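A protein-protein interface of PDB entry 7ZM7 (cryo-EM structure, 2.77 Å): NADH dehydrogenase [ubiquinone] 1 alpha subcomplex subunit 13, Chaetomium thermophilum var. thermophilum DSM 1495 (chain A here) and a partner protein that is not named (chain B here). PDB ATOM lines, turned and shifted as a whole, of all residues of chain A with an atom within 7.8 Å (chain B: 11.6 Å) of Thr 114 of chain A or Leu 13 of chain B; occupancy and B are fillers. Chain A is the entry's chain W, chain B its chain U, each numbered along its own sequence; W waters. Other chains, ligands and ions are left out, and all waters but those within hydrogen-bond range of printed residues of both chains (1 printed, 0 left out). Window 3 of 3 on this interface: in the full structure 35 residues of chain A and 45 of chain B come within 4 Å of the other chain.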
ATOM      1  N   ASP A  78      21.335  18.374 -11.367  1.00  0.00           N
ATOM      2  CA  ASP A  78      21.619  19.524 -12.265  1.00  0.00           C
ATOM      3  C   ASP A  78      22.175  19.030 -13.609  1.00  0.00           C
ATOM      4  O   ASP A  78      21.852  19.642 -14.620  1.00  0.00           O
ATOM      5  CB  ASP A  78      22.510  20.525 -11.535  1.00  0.00           C
ATOM      6  CG  ASP A  78      22.545  21.907 -12.155  1.00  0.00           C
ATOM      7  OD1 ASP A  78      21.573  22.657 -11.948  1.00  0.00           O
ATOM      8  OD2 ASP A  78      23.547  22.227 -12.820  1.00  0.00           O
ATOM      9  N   ARG A  81      19.202  17.726 -15.363  1.00  0.00           N
ATOM     10  CA  ARG A  81      18.346  18.827 -15.781  1.00  0.00           C
ATOM     11  C   ARG A  81      18.859  19.494 -17.052  1.00  0.00           C
ATOM     12  O   ARG A  81      18.107  19.696 -18.009  1.00  0.00           O
ATOM     13  CB  ARG A  81      18.240  19.840 -14.648  1.00  0.00           C
ATOM     14  CG  ARG A  81      17.243  20.931 -14.860  1.00  0.00           C
ATOM     15  CD  ARG A  81      17.206  21.874 -13.684  1.00  0.00           C
ATOM     16  NE  ARG A  81      18.493  22.503 -13.456  1.00  0.00           N
ATOM     17  CZ  ARG A  81      18.931  23.559 -14.121  1.00  0.00           C
ATOM     18  NH1 ARG A  81      20.118  24.071 -13.851  1.00  0.00           N
ATOM     19  NH2 ARG A  81      18.165  24.109 -15.041  1.00  0.00           N
ATOM     20  N   ARG A  82      20.141  19.843 -17.086  1.00  0.00           N
ATOM     21  CA  ARG A  82      20.662  20.567 -18.235  1.00  0.00           C
ATOM     22  C   ARG A  82      20.847  19.661 -19.436  1.00  0.00           C
ATOM     23  O   ARG A  82      20.799  20.137 -20.571  1.00  0.00           O
ATOM     24  CB  ARG A  82      21.972  21.253 -17.875  1.00  0.00           C
ATOM     25  CG  ARG A  82      21.833  22.235 -16.745  1.00  0.00           C
ATOM     26  CD  ARG A  82      23.078  23.024 -16.544  1.00  0.00           C
ATOM     27  NE  ARG A  82      23.409  23.844 -17.694  1.00  0.00           N
ATOM     28  CZ  ARG A  82      23.831  25.091 -17.599  1.00  0.00           C
ATOM     29  NH1 ARG A  82      24.112  25.783 -18.679  1.00  0.00           N
ATOM     30  NH2 ARG A  82      23.967  25.638 -16.410  1.00  0.00           N
ATOM     31  N   PHE A 111      31.401  21.525 -24.862  1.00  0.00           N
ATOM     32  CA  PHE A 111      30.921  22.728 -25.513  1.00  0.00           C
ATOM     33  C   PHE A 111      29.462  22.952 -25.145  1.00  0.00           C
ATOM     34  O   PHE A 111      28.700  22.010 -24.924  1.00  0.00           O
ATOM     35  CB  PHE A 111      31.057  22.621 -27.020  1.00  0.00           C
ATOM     36  CG  PHE A 111      32.450  22.422 -27.496  1.00  0.00           C
ATOM     37  CD1 PHE A 111      33.388  23.425 -27.376  1.00  0.00           C
ATOM     38  CD2 PHE A 111      32.808  21.254 -28.139  1.00  0.00           C
ATOM     39  CE1 PHE A 111      34.659  23.246 -27.857  1.00  0.00           C
ATOM     40  CE2 PHE A 111      34.077  21.067 -28.598  1.00  0.00           C
ATOM     41  CZ  PHE A 111      35.003  22.061 -28.459  1.00  0.00           C
ATOM     42  N   ALA A 112      29.079  24.219 -25.087  1.00  0.00           N
ATOM     43  CA  ALA A 112      27.704  24.597 -24.804  1.00  0.00           C
ATOM     44  C   ALA A 112      27.221  25.582 -25.854  1.00  0.00           C
ATOM     45  O   ALA A 112      28.003  26.329 -26.442  1.00  0.00           O
ATOM     46  CB  ALA A 112      27.553  25.216 -23.409  1.00  0.00           C
ATOM     47  N   VAL A 113      25.936  25.553 -26.100  1.00  0.00           N
ATOM     48  CA  VAL A 113      25.288  26.593 -26.882  1.00  0.00           C
ATOM     49  C   VAL A 113      25.028  27.778 -25.974  1.00  0.00           C
ATOM     50  O   VAL A 113      24.477  27.636 -24.881  1.00  0.00           O
ATOM     51  CB  VAL A 113      23.998  26.055 -27.517  1.00  0.00           C
ATOM     52  CG1 VAL A 113      23.200  27.145 -28.125  1.00  0.00           C
ATOM     53  CG2 VAL A 113      24.366  25.069 -28.564  1.00  0.00           C
ATOM     54  N   THR A 114      25.458  28.948 -26.411  1.00  0.00           N
ATOM     55  CA  THR A 114      25.357  30.147 -25.610  1.00  0.00           C
ATOM     56  C   THR A 114      24.604  31.194 -26.406  1.00  0.00           C
ATOM     57  O   THR A 114      24.535  31.111 -27.638  1.00  0.00           O
ATOM     58  CB  THR A 114      26.730  30.705 -25.200  1.00  0.00           C
ATOM     59  OG1 THR A 114      27.621  30.660 -26.308  1.00  0.00           O
ATOM     60  CG2 THR A 114      27.321  29.930 -24.058  1.00  0.00           C
ATOM     61  N   PRO A 115      24.014  32.177 -25.732  1.00  0.00           N
ATOM     62  CA  PRO A 115      23.529  33.359 -26.438  1.00  0.00           C
ATOM     63  C   PRO A 115      24.668  34.103 -27.105  1.00  0.00           C
ATOM     64  O   PRO A 115      25.835  33.995 -26.730  1.00  0.00           O
ATOM     65  CB  PRO A 115      22.891  34.205 -25.341  1.00  0.00           C
ATOM     66  CG  PRO A 115      22.748  33.314 -24.184  1.00  0.00           C
ATOM     67  CD  PRO A 115      23.712  32.215 -24.299  1.00  0.00           C
ATOM     68  N   SER A 116      24.311  34.857 -28.133  1.00  0.00           N
ATOM     69  CA  SER A 116      25.297  35.687 -28.799  1.00  0.00           C
ATOM     70  C   SER A 116      25.688  36.897 -27.959  1.00  0.00           C
ATOM     71  O   SER A 116      26.721  37.514 -28.225  1.00  0.00           O
ATOM     72  CB  SER A 116      24.766  36.094 -30.169  1.00  0.00           C
ATOM     73  OG  SER A 116      23.417  36.506 -30.075  1.00  0.00           O
ATOM     74  N   LYS A 117      24.903  37.246 -26.941  1.00  0.00           N
ATOM     75  CA  LYS A 117      25.234  38.384 -26.097  1.00  0.00           C
ATOM     76  C   LYS A 117      25.004  38.086 -24.624  1.00  0.00           C
ATOM     77  O   LYS A 117      24.109  37.318 -24.267  1.00  0.00           O
ATOM     78  CB  LYS A 117      24.406  39.617 -26.486  1.00  0.00           C
ATOM     79  CG  LYS A 117      24.708  40.163 -27.874  1.00  0.00           C
ATOM     80  CD  LYS A 117      26.130  40.686 -27.961  1.00  0.00           C
ATOM     81  CE  LYS A 117      26.270  42.020 -27.252  1.00  0.00           C
ATOM     82  NZ  LYS A 117      25.508  43.093 -27.948  1.00  0.00           N
ATOM     83  N   MET B   1      28.982  19.745 -17.302  1.00  0.00           N
ATOM     84  CA  MET B   1      30.084  20.297 -18.065  1.00  0.00           C
ATOM     85  C   MET B   1      31.383  19.693 -17.592  1.00  0.00           C
ATOM     86  O   MET B   1      31.417  19.070 -16.539  1.00  0.00           O
ATOM     87  CB  MET B   1      30.105  21.799 -17.921  1.00  0.00           C
ATOM     88  N   ALA B   2      32.445  19.896 -18.370  1.00  0.00           N
ATOM     89  CA  ALA B   2      33.716  19.181 -18.118  1.00  0.00           C
ATOM     90  C   ALA B   2      34.235  19.455 -16.711  1.00  0.00           C
ATOM     91  O   ALA B   2      33.920  20.513 -16.168  1.00  0.00           O
ATOM     92  CB  ALA B   2      34.718  19.594 -19.163  1.00  0.00           C
ATOM     93  N   PRO B   6      39.098  25.793 -14.795  1.00  0.00           N
ATOM     94  CA  PRO B   6      39.119  26.796 -15.848  1.00  0.00           C
ATOM     95  C   PRO B   6      40.217  27.856 -15.673  1.00  0.00           C
ATOM     96  O   PRO B   6      40.514  28.201 -14.554  1.00  0.00           O
ATOM     97  CB  PRO B   6      37.697  27.350 -15.761  1.00  0.00           C
ATOM     98  CG  PRO B   6      37.333  27.256 -14.298  1.00  0.00           C
ATOM     99  CD  PRO B   6      38.135  26.100 -13.741  1.00  0.00           C
ATOM    100  N   ASN B   9      38.126  31.706 -17.828  1.00  0.00           N
ATOM    101  CA  ASN B   9      36.655  31.884 -17.717  1.00  0.00           C
ATOM    102  C   ASN B   9      36.319  33.339 -17.379  1.00  0.00           C
ATOM    103  O   ASN B   9      36.924  33.882 -16.457  1.00  0.00           O
ATOM    104  CB  ASN B   9      36.047  30.933 -16.690  1.00  0.00           C
ATOM    105  CG  ASN B   9      36.825  30.852 -15.394  1.00  0.00           C
ATOM    106  OD1 ASN B   9      38.048  30.745 -15.393  1.00  0.00           O
ATOM    107  ND2 ASN B   9      36.120  30.898 -14.280  1.00  0.00           N
ATOM    108  N   GLN B  10      35.375  33.934 -18.106  1.00  0.00           N
ATOM    109  CA  GLN B  10      34.959  35.336 -17.851  1.00  0.00           C
ATOM    110  C   GLN B  10      33.431  35.415 -17.738  1.00  0.00           C
ATOM    111  O   GLN B  10      32.947  36.449 -17.264  1.00  0.00           O
ATOM    112  CB  GLN B  10      35.486  36.250 -18.958  1.00  0.00           C
ATOM    113  CG  GLN B  10      37.004  36.278 -19.062  1.00  0.00           C
ATOM    114  CD  GLN B  10      37.658  36.916 -17.862  1.00  0.00           C
ATOM    115  OE1 GLN B  10      37.202  37.933 -17.349  1.00  0.00           O
ATOM    116  NE2 GLN B  10      38.747  36.323 -17.409  1.00  0.00           N
ATOM    117  N   HIS B  11      32.712  34.360 -18.135  1.00  0.00           N
ATOM    118  CA  HIS B  11      31.221  34.376 -18.136  1.00  0.00           C
ATOM    119  C   HIS B  11      30.612  33.114 -17.507  1.00  0.00           C
ATOM    120  O   HIS B  11      31.317  32.117 -17.417  1.00  0.00           O
ATOM    121  CB  HIS B  11      30.655  34.595 -19.556  1.00  0.00           C
ATOM    122  CG  HIS B  11      31.072  35.843 -20.251  1.00  0.00           C
ATOM    123  ND1 HIS B  11      30.643  37.089 -19.852  1.00  0.00           N
ATOM    124  CD2 HIS B  11      31.828  36.037 -21.350  1.00  0.00           C
ATOM    125  CE1 HIS B  11      31.143  38.002 -20.655  1.00  0.00           C
ATOM    126  NE2 HIS B  11      31.872  37.381 -21.583  1.00  0.00           N
ATOM    127  N   VAL B  12      29.354  33.175 -17.059  1.00  0.00           N
ATOM    128  CA  VAL B  12      28.623  32.045 -16.496  1.00  0.00           C
ATOM    129  C   VAL B  12      27.399  31.788 -17.356  1.00  0.00           C
ATOM    130  O   VAL B  12      26.735  32.734 -17.787  1.00  0.00           O
ATOM    131  CB  VAL B  12      28.225  32.300 -15.033  1.00  0.00           C
ATOM    132  CG1 VAL B  12      27.155  31.339 -14.610  1.00  0.00           C
ATOM    133  CG2 VAL B  12      29.436  32.143 -14.133  1.00  0.00           C
ATOM    134  N   LEU B  13      27.111  30.519 -17.624  1.00  0.00           N
ATOM    135  CA  LEU B  13      25.949  30.131 -18.413  1.00  0.00           C
ATOM    136  C   LEU B  13      24.938  29.403 -17.535  1.00  0.00           C
ATOM    137  O   LEU B  13      25.173  28.267 -17.120  1.00  0.00           O
ATOM    138  CB  LEU B  13      26.358  29.266 -19.594  1.00  0.00           C
ATOM    139  CG  LEU B  13      25.218  28.646 -20.385  1.00  0.00           C
ATOM    140  CD1 LEU B  13      24.418  29.688 -21.124  1.00  0.00           C
ATOM    141  CD2 LEU B  13      25.779  27.658 -21.340  1.00  0.00           C
ATOM    142  N   LEU B  14      23.789  30.035 -17.297  1.00  0.00           N
ATOM    143  CA  LEU B  14      22.715  29.483 -16.433  1.00  0.00           C
ATOM    144  C   LEU B  14      21.597  28.919 -17.308  1.00  0.00           C
ATOM    145  O   LEU B  14      21.353  29.482 -18.369  1.00  0.00           O
ATOM    146  CB  LEU B  14      22.187  30.580 -15.504  1.00  0.00           C
ATOM    147  CG  LEU B  14      23.064  30.946 -14.310  1.00  0.00           C
ATOM    148  CD1 LEU B  14      22.248  31.683 -13.264  1.00  0.00           C
ATOM    149  CD2 LEU B  14      23.686  29.706 -13.698  1.00  0.00           C
ATOM    150  N   ASP B  15      21.027  27.779 -16.941  1.00  0.00           N
ATOM    151  CA  ASP B  15      19.853  27.268 -17.701  1.00  0.00           C
ATOM    152  C   ASP B  15      18.638  27.300 -16.769  1.00  0.00           C
ATOM    153  O   ASP B  15      18.676  26.618 -15.750  1.00  0.00           O
ATOM    154  CB  ASP B  15      20.137  25.893 -18.315  1.00  0.00           C
ATOM    155  CG  ASP B  15      19.321  25.613 -19.557  1.00  0.00           C
ATOM    156  OD1 ASP B  15      18.598  26.521 -19.988  1.00  0.00           O
ATOM    157  OD2 ASP B  15      19.418  24.488 -20.080  1.00  0.00           O
ATOM    158  N   THR B  16      17.618  28.095 -17.095  1.00  0.00           N
ATOM    159  CA  THR B  16      16.454  28.248 -16.180  1.00  0.00           C
ATOM    160  C   THR B  16      15.438  27.132 -16.433  1.00  0.00           C
ATOM    161  O   THR B  16      14.412  27.102 -15.734  1.00  0.00           O
ATOM    162  CB  THR B  16      15.821  29.637 -16.307  1.00  0.00           C
ATOM    163  OG1 THR B  16      15.207  29.719 -17.595  1.00  0.00           O
ATOM    164  CG2 THR B  16      16.820  30.757 -16.129  1.00  0.00           C
ATOM    165  N   THR B  17      15.729  26.243 -17.383  1.00  0.00           N
ATOM    166  CA  THR B  17      14.797  25.141 -17.721  1.00  0.00           C
ATOM    167  C   THR B  17      14.656  24.229 -16.502  1.00  0.00           C
ATOM    168  O   THR B  17      15.684  23.856 -15.934  1.00  0.00           O
ATOM    169  CB  THR B  17      15.302  24.391 -18.959  1.00  0.00           C
ATOM    170  OG1 THR B  17      15.944  25.329 -19.821  1.00  0.00           O
ATOM    171  CG2 THR B  17      14.200  23.674 -19.707  1.00  0.00           C
HETATM  172  O   HOH W   1      22.679  23.342 -20.528  1.00  0.00           O
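O of Leu 13 of chain B is in hydrogen-bond range of NH2 of Arg 82 of chain A, at 3.0 Å. The backbone carbonyl oxygen (O) of Asp 15 of chain B is in hydrogen-bond range of the guanidinium group (NH2) of Arg 81 of chain A, at 2.7 Å. O of Thr 17 of chain B is in hydrogen-bond range of NH2 of Arg 81 of chain A (2.6 Å).
OD1 of Asp 78 of chain A is in salt-bridge range of NH1 of Arg 81 of chain A. OD1 of Asp 15 of chain B sits at hydrogen-bond distance from OG1 of Thr 17 of chain B, 2.9 Å away.
Arg 82 of chain A touches Asp 15 of chain B. Leu 13 of chain B touches Ala 112 of chain A. Leu 13 of chain B touches Val 113 of chain A (CD2 to O, 3.8 Å). Thr 114 of chain A touches Leu 13 of chain B.
Of the printed residues of chain B, Arg 81 of chain A touches Asp 15 (2.7 Å) and Thr 17 (2.6 Å). Of the printed residues of chain B, Arg 82 of chain A touches Leu 13 and Asp 15. Ala 112 of chain A touches just one residue of chain B: Leu 13. Ser 116 of chain A touches none of the printed residues of chain B. Val 12 of chain B touches none of the printed residues of chain A. Of the printed residues of chain A, Leu 13 of chain B touches Arg 82 (3.0 Å), Ala 112 (3.7 Å), Val 113 (3.8 Å) and Thr 114 (3.9 Å). Printed residues of chain A within 4 Å of Asp 15 of chain B: Arg 81 (2.7 Å) and Arg 82 (3.7 Å). Thr 16 of chain B touches none of the printed residues of chain A. Printed residues of chain A within 4 Å of Thr 17 of chain B: Arg 81 (2.6 Å). The nearest residue of chain B that does not touch Thr 114 of chain A is Val 12 of chain B (6.9 Å). The nearest residue of chain A that does not touch Leu 13 of chain B is Pro 115 of chain A (4.1 Å).
Of the 12 printed residues of chain B, 3 touch a printed residue of chain A. Printed residues of chain B that touch a printed residue of chain A: Leu 13, Asp 15 and Thr 17. Hydrophobic or aromatic side chains of chain B within 4 Å of the printed part of chain A: Leu 13. Of the 10 printed residues of chain A, 5 touch a printed residue of chain B. Printed residues of chain A that touch a printed residue of chain B: Arg 81, Arg 82, Ala 112, Val 113 and Thr 114. Among the printed residues, 7 pairs touch across the chains. Among the printed residues, no Asp or Glu carboxylate lies within 4 Å of a Lys or Arg side-chain nitrogen of the other chain.
Water W1 lies within hydrogen-bond range of NE of Arg 82 of chain A and OD2 of Asp 15 of chain B.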
